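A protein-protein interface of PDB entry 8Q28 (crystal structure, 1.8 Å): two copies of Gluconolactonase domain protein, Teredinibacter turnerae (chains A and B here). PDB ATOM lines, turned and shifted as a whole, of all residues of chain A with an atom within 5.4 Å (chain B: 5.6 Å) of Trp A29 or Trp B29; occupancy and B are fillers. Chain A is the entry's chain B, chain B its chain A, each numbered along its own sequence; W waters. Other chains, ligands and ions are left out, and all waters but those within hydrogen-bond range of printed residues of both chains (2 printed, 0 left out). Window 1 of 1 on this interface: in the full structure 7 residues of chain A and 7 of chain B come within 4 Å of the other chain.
Of chain B, only Trp B29 comes within 4 Å of Trp A29. Trp B29 touches one residue of chain A. Printed residues of chain B within 4 Å of Gly A28: Gln B112. Of the printed residues of chain B, Gln A30 touches Gln B112. Printed residues of chain A within 4 Å of Gln B112: Gly A28 (3.1 Å) and Gln A30 (3.1 Å). Phe A26 touches none of the printed residues of chain B. Ala B113 touches none of the printed residues of chain A. The nearest printed residue of chain A that does not touch Trp B29 is Gly A28 (5.7 Å).
Of the 13 printed residues of chain A, 3 touch a printed residue of chain B. Hydrophobic or aromatic side chains of chain A that line the printed part of chain B: Trp A29. Of the 14 printed residues of chain B, 2 touch a printed residue of chain A. Hydrophobic or aromatic side chains of chain B that line the printed part of chain A: Trp B29. Among the printed residues, 3 pairs touch across the chains.
N of Gly A28 sits at hydrogen-bond distance from O of Pro A66, 2.9 Å away.
The side-chain amide nitrogen of Gln B112 lies within hydrogen-bond range of the backbone carbonyl oxygen of Gly A28. NE2 of Gln B112 sits at hydrogen-bond distance from OE1 of Gln A30 (3.1 Å).
Trp A29 touches its own counterpart, Trp B29. Positions printed for both chains: 26, 27, 28, 29, 30, 31, 64, 65, 66, 111, 113, 213 and 215. Of the 3 pairs that touch across the chains among the printed residues, 1 has its exchanged pair printed and touching as well.
Water W1 lies within hydrogen-bond range of the backbone carbonyl oxygen of Trp A29 (2.8 Å) and the backbone carbonyl oxygen of Trp B29 (2.9 Å). Water W2 lies within hydrogen-bond range of the backbone NH (N) of Ala B113 (2.8 Å), the side-chain amide oxygen (OE1) of Gln B112 (2.8 Å) and the backbone carbonyl oxygen (O) of Gly A28 (3.4 Å).
Trp B29 touches Trp A29.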
ATOM      1  N   PHE A  26     -11.794 -18.470  -5.475  1.00  0.00           N
ATOM      2  CA  PHE A  26     -10.431 -18.750  -5.068  1.00  0.00           C
ATOM      3  C   PHE A  26     -10.517 -19.026  -3.567  1.00  0.00           C
ATOM      4  O   PHE A  26     -10.722 -18.084  -2.783  1.00  0.00           O
ATOM      5  CB  PHE A  26      -9.503 -17.601  -5.421  1.00  0.00           C
ATOM      6  CG  PHE A  26      -8.008 -17.878  -5.290  1.00  0.00           C
ATOM      7  CD1 PHE A  26      -7.327 -18.610  -6.266  1.00  0.00           C
ATOM      8  CD2 PHE A  26      -7.299 -17.465  -4.178  1.00  0.00           C
ATOM      9  CE1 PHE A  26      -5.979 -18.890  -6.131  1.00  0.00           C
ATOM     10  CE2 PHE A  26      -5.921 -17.651  -4.080  1.00  0.00           C
ATOM     11  CZ  PHE A  26      -5.266 -18.444  -5.018  1.00  0.00           C
ATOM     12  N   VAL A  27     -10.487 -20.313  -3.262  1.00  0.00           N
ATOM     13  CA  VAL A  27     -10.792 -20.792  -1.932  1.00  0.00           C
ATOM     14  C   VAL A  27      -9.689 -21.744  -1.548  1.00  0.00           C
ATOM     15  O   VAL A  27      -9.428 -22.665  -2.299  1.00  0.00           O
ATOM     16  CB  VAL A  27     -12.177 -21.428  -1.926  1.00  0.00           C
ATOM     17  CG1 VAL A  27     -12.445 -22.233  -0.623  1.00  0.00           C
ATOM     18  CG2 VAL A  27     -13.245 -20.396  -2.222  1.00  0.00           C
ATOM     19  N   GLY A  28      -9.074 -21.538  -0.369  1.00  0.00           N
ATOM     20  CA  GLY A  28      -8.027 -22.460   0.053  1.00  0.00           C
ATOM     21  C   GLY A  28      -6.843 -22.521  -0.887  1.00  0.00           C
ATOM     22  O   GLY A  28      -6.255 -23.599  -0.974  1.00  0.00           O
ATOM     23  N   TRP A  29      -6.522 -21.412  -1.556  1.00  0.00           N
ATOM     24  CA  TRP A  29      -5.388 -21.216  -2.443  1.00  0.00           C
ATOM     25  C   TRP A  29      -5.597 -21.929  -3.780  1.00  0.00           C
ATOM     26  O   TRP A  29      -4.624 -22.144  -4.505  1.00  0.00           O
ATOM     27  CB  TRP A  29      -4.091 -21.703  -1.792  1.00  0.00           C
ATOM     28  CG  TRP A  29      -3.695 -20.966  -0.544  1.00  0.00           C
ATOM     29  CD1 TRP A  29      -3.895 -21.363   0.737  1.00  0.00           C
ATOM     30  CD2 TRP A  29      -3.112 -19.659  -0.476  1.00  0.00           C
ATOM     31  NE1 TRP A  29      -3.400 -20.432   1.582  1.00  0.00           N
ATOM     32  CE2 TRP A  29      -2.917 -19.377   0.883  1.00  0.00           C
ATOM     33  CE3 TRP A  29      -2.699 -18.711  -1.403  1.00  0.00           C
ATOM     34  CZ2 TRP A  29      -2.317 -18.233   1.331  1.00  0.00           C
ATOM     35  CZ3 TRP A  29      -2.061 -17.577  -0.945  1.00  0.00           C
ATOM     36  CH2 TRP A  29      -1.871 -17.339   0.379  1.00  0.00           C
ATOM     37  N   GLN A  30      -6.817 -22.338  -4.066  1.00  0.00           N
ATOM     38  CA  GLN A  30      -7.088 -23.008  -5.337  1.00  0.00           C
ATOM     39  C   GLN A  30      -8.212 -22.278  -6.079  1.00  0.00           C
ATOM     40  O   GLN A  30      -9.305 -22.046  -5.536  1.00  0.00           O
ATOM     41  CB  GLN A  30      -7.386 -24.473  -5.029  1.00  0.00           C
ATOM     42  CG  GLN A  30      -7.826 -25.220  -6.249  1.00  0.00           C
ATOM     43  CD  GLN A  30      -8.059 -26.665  -5.930  1.00  0.00           C
ATOM     44  OE1 GLN A  30      -8.323 -27.028  -4.787  1.00  0.00           O
ATOM     45  NE2 GLN A  30      -8.064 -27.453  -6.990  1.00  0.00           N
ATOM     46  N   SER A  31      -7.946 -21.980  -7.374  1.00  0.00           N
ATOM     47  CA  SER A  31      -8.901 -21.402  -8.287  1.00  0.00           C
ATOM     48  C   SER A  31      -9.978 -22.445  -8.643  1.00  0.00           C
ATOM     49  O   SER A  31      -9.636 -23.584  -8.980  1.00  0.00           O
ATOM     50  CB  SER A  31      -8.195 -20.981  -9.551  1.00  0.00           C
ATOM     51  OG  SER A  31      -9.067 -20.476 -10.509  1.00  0.00           O
ATOM     52  N   ALA A  64      -6.138 -17.106   6.996  1.00  0.00           N
ATOM     53  CA  ALA A  64      -4.884 -17.248   6.278  1.00  0.00           C
ATOM     54  C   ALA A  64      -5.148 -17.980   4.974  1.00  0.00           C
ATOM     55  O   ALA A  64      -4.467 -17.712   3.981  1.00  0.00           O
ATOM     56  CB  ALA A  64      -3.953 -18.076   7.104  1.00  0.00           C
ATOM     57  N   ALA A  65      -6.129 -18.901   5.013  1.00  0.00           N
ATOM     58  CA  ALA A  65      -6.601 -19.542   3.797  1.00  0.00           C
ATOM     59  C   ALA A  65      -7.641 -18.669   3.147  1.00  0.00           C
ATOM     60  O   ALA A  65      -8.621 -18.289   3.816  1.00  0.00           O
ATOM     61  CB  ALA A  65      -7.232 -20.863   4.086  1.00  0.00           C
ATOM     62  N   PRO A  66      -7.477 -18.221   1.875  1.00  0.00           N
ATOM     63  CA  PRO A  66      -8.401 -17.230   1.337  1.00  0.00           C
ATOM     64  C   PRO A  66      -9.743 -17.814   0.976  1.00  0.00           C
ATOM     65  O   PRO A  66      -9.902 -18.981   0.613  1.00  0.00           O
ATOM     66  CB  PRO A  66      -7.709 -16.709   0.090  1.00  0.00           C
ATOM     67  CG  PRO A  66      -6.886 -17.949  -0.360  1.00  0.00           C
ATOM     68  CD  PRO A  66      -6.393 -18.512   0.946  1.00  0.00           C
ATOM     69  N   ALA A 111      -4.958 -18.747 -11.600  1.00  0.00           N
ATOM     70  CA  ALA A 111      -4.569 -19.899 -10.758  1.00  0.00           C
ATOM     71  C   ALA A 111      -3.803 -19.522  -9.488  1.00  0.00           C
ATOM     72  O   ALA A 111      -3.596 -20.366  -8.597  1.00  0.00           O
ATOM     73  CB  ALA A 111      -3.644 -20.771 -11.605  1.00  0.00           C
ATOM     74  N   ALA A 113      -2.255 -16.345  -6.502  1.00  0.00           N
ATOM     75  CA  ALA A 113      -2.380 -15.050  -5.813  1.00  0.00           C
ATOM     76  C   ALA A 113      -1.043 -14.293  -5.837  1.00  0.00           C
ATOM     77  O   ALA A 113      -0.608 -13.549  -4.962  1.00  0.00           O
ATOM     78  CB  ALA A 113      -2.869 -15.318  -4.424  1.00  0.00           C
ATOM     79  N   HIS A 213      -8.938 -12.462   2.904  1.00  0.00           N
ATOM     80  CA  HIS A 213      -7.593 -13.085   2.808  1.00  0.00           C
ATOM     81  C   HIS A 213      -6.666 -12.399   3.788  1.00  0.00           C
ATOM     82  O   HIS A 213      -6.294 -11.248   3.605  1.00  0.00           O
ATOM     83  CB  HIS A 213      -7.088 -13.023   1.381  1.00  0.00           C
ATOM     84  CG  HIS A 213      -5.899 -13.923   1.111  1.00  0.00           C
ATOM     85  ND1 HIS A 213      -5.286 -14.051  -0.134  1.00  0.00           N
ATOM     86  CD2 HIS A 213      -5.249 -14.734   1.968  1.00  0.00           C
ATOM     87  CE1 HIS A 213      -4.295 -14.940  -0.015  1.00  0.00           C
ATOM     88  NE2 HIS A 213      -4.286 -15.407   1.260  1.00  0.00           N
ATOM     89  N   PHE A 215      -2.999 -12.192   5.797  1.00  0.00           N
ATOM     90  CA  PHE A 215      -1.600 -12.551   6.004  1.00  0.00           C
ATOM     91  C   PHE A 215      -1.143 -12.230   7.436  1.00  0.00           C
ATOM     92  O   PHE A 215       0.070 -12.201   7.678  1.00  0.00           O
ATOM     93  CB  PHE A 215      -0.707 -11.855   4.973  1.00  0.00           C
ATOM     94  CG  PHE A 215      -0.907 -12.380   3.561  1.00  0.00           C
ATOM     95  CD1 PHE A 215      -2.041 -12.069   2.847  1.00  0.00           C
ATOM     96  CD2 PHE A 215      -0.053 -13.320   3.026  1.00  0.00           C
ATOM     97  CE1 PHE A 215      -2.220 -12.571   1.562  1.00  0.00           C
ATOM     98  CE2 PHE A 215      -0.201 -13.802   1.739  1.00  0.00           C
ATOM     99  CZ  PHE A 215      -1.323 -13.454   1.029  1.00  0.00           C
ATOM    100  N   PHE B  26       5.683 -28.312  -4.922  1.00  0.00           N
ATOM    101  CA  PHE B  26       4.563 -27.540  -4.430  1.00  0.00           C
ATOM    102  C   PHE B  26       5.171 -26.230  -3.919  1.00  0.00           C
ATOM    103  O   PHE B  26       5.819 -26.207  -2.847  1.00  0.00           O
ATOM    104  CB  PHE B  26       3.756 -28.306  -3.379  1.00  0.00           C
ATOM    105  CG  PHE B  26       2.466 -27.663  -2.906  1.00  0.00           C
ATOM    106  CD1 PHE B  26       1.304 -27.870  -3.599  1.00  0.00           C
ATOM    107  CD2 PHE B  26       2.410 -26.928  -1.751  1.00  0.00           C
ATOM    108  CE1 PHE B  26       0.129 -27.323  -3.110  1.00  0.00           C
ATOM    109  CE2 PHE B  26       1.240 -26.433  -1.212  1.00  0.00           C
ATOM    110  CZ  PHE B  26       0.088 -26.612  -1.933  1.00  0.00           C
ATOM    111  N   VAL B  27       5.021 -25.191  -4.767  1.00  0.00           N
ATOM    112  CA  VAL B  27       5.755 -23.947  -4.556  1.00  0.00           C
ATOM    113  C   VAL B  27       4.749 -22.789  -4.630  1.00  0.00           C
ATOM    114  O   VAL B  27       3.997 -22.736  -5.574  1.00  0.00           O
ATOM    115  CB  VAL B  27       6.864 -23.824  -5.610  1.00  0.00           C
ATOM    116  CG1 VAL B  27       7.458 -22.411  -5.706  1.00  0.00           C
ATOM    117  CG2 VAL B  27       7.929 -24.923  -5.449  1.00  0.00           C
ATOM    118  N   GLY B  28       4.700 -21.961  -3.588  1.00  0.00           N
ATOM    119  CA  GLY B  28       3.735 -20.865  -3.543  1.00  0.00           C
ATOM    120  C   GLY B  28       2.313 -21.362  -3.760  1.00  0.00           C
ATOM    121  O   GLY B  28       1.517 -20.656  -4.395  1.00  0.00           O
ATOM    122  N   TRP B  29       1.976 -22.511  -3.169  1.00  0.00           N
ATOM    123  CA  TRP B  29       0.628 -23.020  -2.967  1.00  0.00           C
ATOM    124  C   TRP B  29       0.106 -23.665  -4.232  1.00  0.00           C
ATOM    125  O   TRP B  29      -1.107 -23.848  -4.357  1.00  0.00           O
ATOM    126  CB  TRP B  29      -0.343 -21.955  -2.483  1.00  0.00           C
ATOM    127  CG  TRP B  29       0.022 -21.297  -1.189  1.00  0.00           C
ATOM    128  CD1 TRP B  29       0.524 -20.065  -0.990  1.00  0.00           C
ATOM    129  CD2 TRP B  29      -0.209 -21.872   0.108  1.00  0.00           C
ATOM    130  NE1 TRP B  29       0.639 -19.831   0.338  1.00  0.00           N
ATOM    131  CE2 TRP B  29       0.175 -20.908   1.039  1.00  0.00           C
ATOM    132  CE3 TRP B  29      -0.786 -23.060   0.573  1.00  0.00           C
ATOM    133  CZ2 TRP B  29       0.058 -21.076   2.392  1.00  0.00           C
ATOM    134  CZ3 TRP B  29      -0.964 -23.191   1.920  1.00  0.00           C
ATOM    135  CH2 TRP B  29      -0.535 -22.240   2.820  1.00  0.00           C
ATOM    136  N   GLN B  30       0.997 -23.847  -5.194  1.00  0.00           N
ATOM    137  CA  GLN B  30       0.628 -24.480  -6.445  1.00  0.00           C
ATOM    138  C   GLN B  30       1.444 -25.754  -6.663  1.00  0.00           C
ATOM    139  O   GLN B  30       2.696 -25.751  -6.688  1.00  0.00           O
ATOM    140  CB  GLN B  30       0.726 -23.486  -7.621  1.00  0.00           C
ATOM    141  CG  GLN B  30       0.860 -24.141  -9.001  1.00  0.00           C
ATOM    142  CD  GLN B  30       0.688 -23.069 -10.053  1.00  0.00           C
ATOM    143  OE1 GLN B  30       1.121 -21.926  -9.876  1.00  0.00           O
ATOM    144  NE2 GLN B  30      -0.026 -23.403 -11.124  1.00  0.00           N
ATOM    145  N   SER B  31       0.718 -26.879  -6.878  1.00  0.00           N
ATOM    146  CA  SER B  31       1.331 -28.091  -7.368  1.00  0.00           C
ATOM    147  C   SER B  31       1.929 -27.911  -8.764  1.00  0.00           C
ATOM    148  O   SER B  31       1.283 -27.348  -9.655  1.00  0.00           O
ATOM    149  CB  SER B  31       0.343 -29.286  -7.408  1.00  0.00           C
ATOM    150  OG  SER B  31       0.945 -30.322  -8.156  1.00  0.00           O
ATOM    151  N   ALA B  64       5.822 -18.272   4.694  1.00  0.00           N
ATOM    152  CA  ALA B  64       4.386 -18.414   4.598  1.00  0.00           C
ATOM    153  C   ALA B  64       4.066 -19.144   3.327  1.00  0.00           C
ATOM    154  O   ALA B  64       3.190 -19.974   3.384  1.00  0.00           O
ATOM    155  CB  ALA B  64       3.674 -17.038   4.662  1.00  0.00           C
ATOM    156  N   ALA B  65       4.652 -18.732   2.198  1.00  0.00           N
ATOM    157  CA  ALA B  65       4.518 -19.457   0.953  1.00  0.00           C
ATOM    158  C   ALA B  65       5.448 -20.678   0.916  1.00  0.00           C
ATOM    159  O   ALA B  65       6.649 -20.524   1.143  1.00  0.00           O
ATOM    160  CB  ALA B  65       4.842 -18.582  -0.219  1.00  0.00           C
ATOM    161  N   PRO B  66       4.927 -21.901   0.684  1.00  0.00           N
ATOM    162  CA  PRO B  66       5.720 -23.107   0.853  1.00  0.00           C
ATOM    163  C   PRO B  66       6.619 -23.286  -0.365  1.00  0.00           C
ATOM    164  O   PRO B  66       6.390 -22.821  -1.458  1.00  0.00           O
ATOM    165  CB  PRO B  66       4.667 -24.259   0.849  1.00  0.00           C
ATOM    166  CG  PRO B  66       3.539 -23.652  -0.060  1.00  0.00           C
ATOM    167  CD  PRO B  66       3.521 -22.215   0.375  1.00  0.00           C
ATOM    168  N   ALA B 111      -2.968 -31.296  -5.181  1.00  0.00           N
ATOM    169  CA  ALA B 111      -3.349 -29.906  -5.443  1.00  0.00           C
ATOM    170  C   ALA B 111      -3.395 -29.054  -4.189  1.00  0.00           C
ATOM    171  O   ALA B 111      -3.331 -27.846  -4.325  1.00  0.00           O
ATOM    172  CB  ALA B 111      -4.744 -29.859  -6.061  1.00  0.00           C
ATOM    173  N   GLN B 112      -3.433 -29.649  -3.006  1.00  0.00           N
ATOM    174  CA  GLN B 112      -3.867 -28.972  -1.806  1.00  0.00           C
ATOM    175  C   GLN B 112      -2.939 -29.222  -0.619  1.00  0.00           C
ATOM    176  O   GLN B 112      -2.642 -30.352  -0.325  1.00  0.00           O
ATOM    177  CB  GLN B 112      -5.267 -29.538  -1.471  1.00  0.00           C
ATOM    178  CG  GLN B 112      -6.448 -28.727  -2.025  1.00  0.00           C
ATOM    179  CD  GLN B 112      -6.521 -27.369  -1.348  1.00  0.00           C
ATOM    180  OE1 GLN B 112      -5.971 -27.176  -0.265  1.00  0.00           O
ATOM    181  NE2 GLN B 112      -7.178 -26.394  -1.965  1.00  0.00           N
ATOM    182  N   ALA B 113      -2.781 -28.235   0.259  1.00  0.00           N
ATOM    183  CA  ALA B 113      -2.096 -28.453   1.533  1.00  0.00           C
ATOM    184  C   ALA B 113      -3.056 -28.704   2.697  1.00  0.00           C
ATOM    185  O   ALA B 113      -2.772 -28.510   3.883  1.00  0.00           O
ATOM    186  CB  ALA B 113      -1.245 -27.259   1.805  1.00  0.00           C
ATOM    187  N   HIS B 213       7.745 -24.746   5.044  1.00  0.00           N
ATOM    188  CA  HIS B 213       6.381 -24.220   5.072  1.00  0.00           C
ATOM    189  C   HIS B 213       6.125 -23.680   6.465  1.00  0.00           C
ATOM    190  O   HIS B 213       6.029 -24.437   7.406  1.00  0.00           O
ATOM    191  CB  HIS B 213       5.416 -25.256   4.479  1.00  0.00           C
ATOM    192  CG  HIS B 213       4.068 -24.644   4.230  1.00  0.00           C
ATOM    193  ND1 HIS B 213       2.992 -25.378   3.805  1.00  0.00           N
ATOM    194  CD2 HIS B 213       3.681 -23.334   4.186  1.00  0.00           C
ATOM    195  CE1 HIS B 213       2.000 -24.561   3.454  1.00  0.00           C
ATOM    196  NE2 HIS B 213       2.344 -23.311   3.770  1.00  0.00           N
ATOM    197  N   PHE B 215       3.750 -21.459   9.105  1.00  0.00           N
ATOM    198  CA  PHE B 215       2.475 -20.874   9.423  1.00  0.00           C
ATOM    199  C   PHE B 215       2.665 -19.821  10.507  1.00  0.00           C
ATOM    200  O   PHE B 215       1.643 -19.432  11.087  1.00  0.00           O
ATOM    201  CB  PHE B 215       1.456 -21.932   9.840  1.00  0.00           C
ATOM    202  CG  PHE B 215       0.885 -22.644   8.633  1.00  0.00           C
ATOM    203  CD1 PHE B 215       1.615 -23.643   7.990  1.00  0.00           C
ATOM    204  CD2 PHE B 215      -0.338 -22.273   8.084  1.00  0.00           C
ATOM    205  CE1 PHE B 215       1.143 -24.286   6.866  1.00  0.00           C
ATOM    206  CE2 PHE B 215      -0.824 -22.932   6.952  1.00  0.00           C
ATOM    207  CZ  PHE B 215      -0.086 -23.917   6.328  1.00  0.00           C
HETATM  208  O   HOH W   1      -3.371 -23.943  -6.189  1.00  0.00           O
HETATM  209  O   HOH W   2      -3.581 -25.666  -0.552  1.00  0.00           O
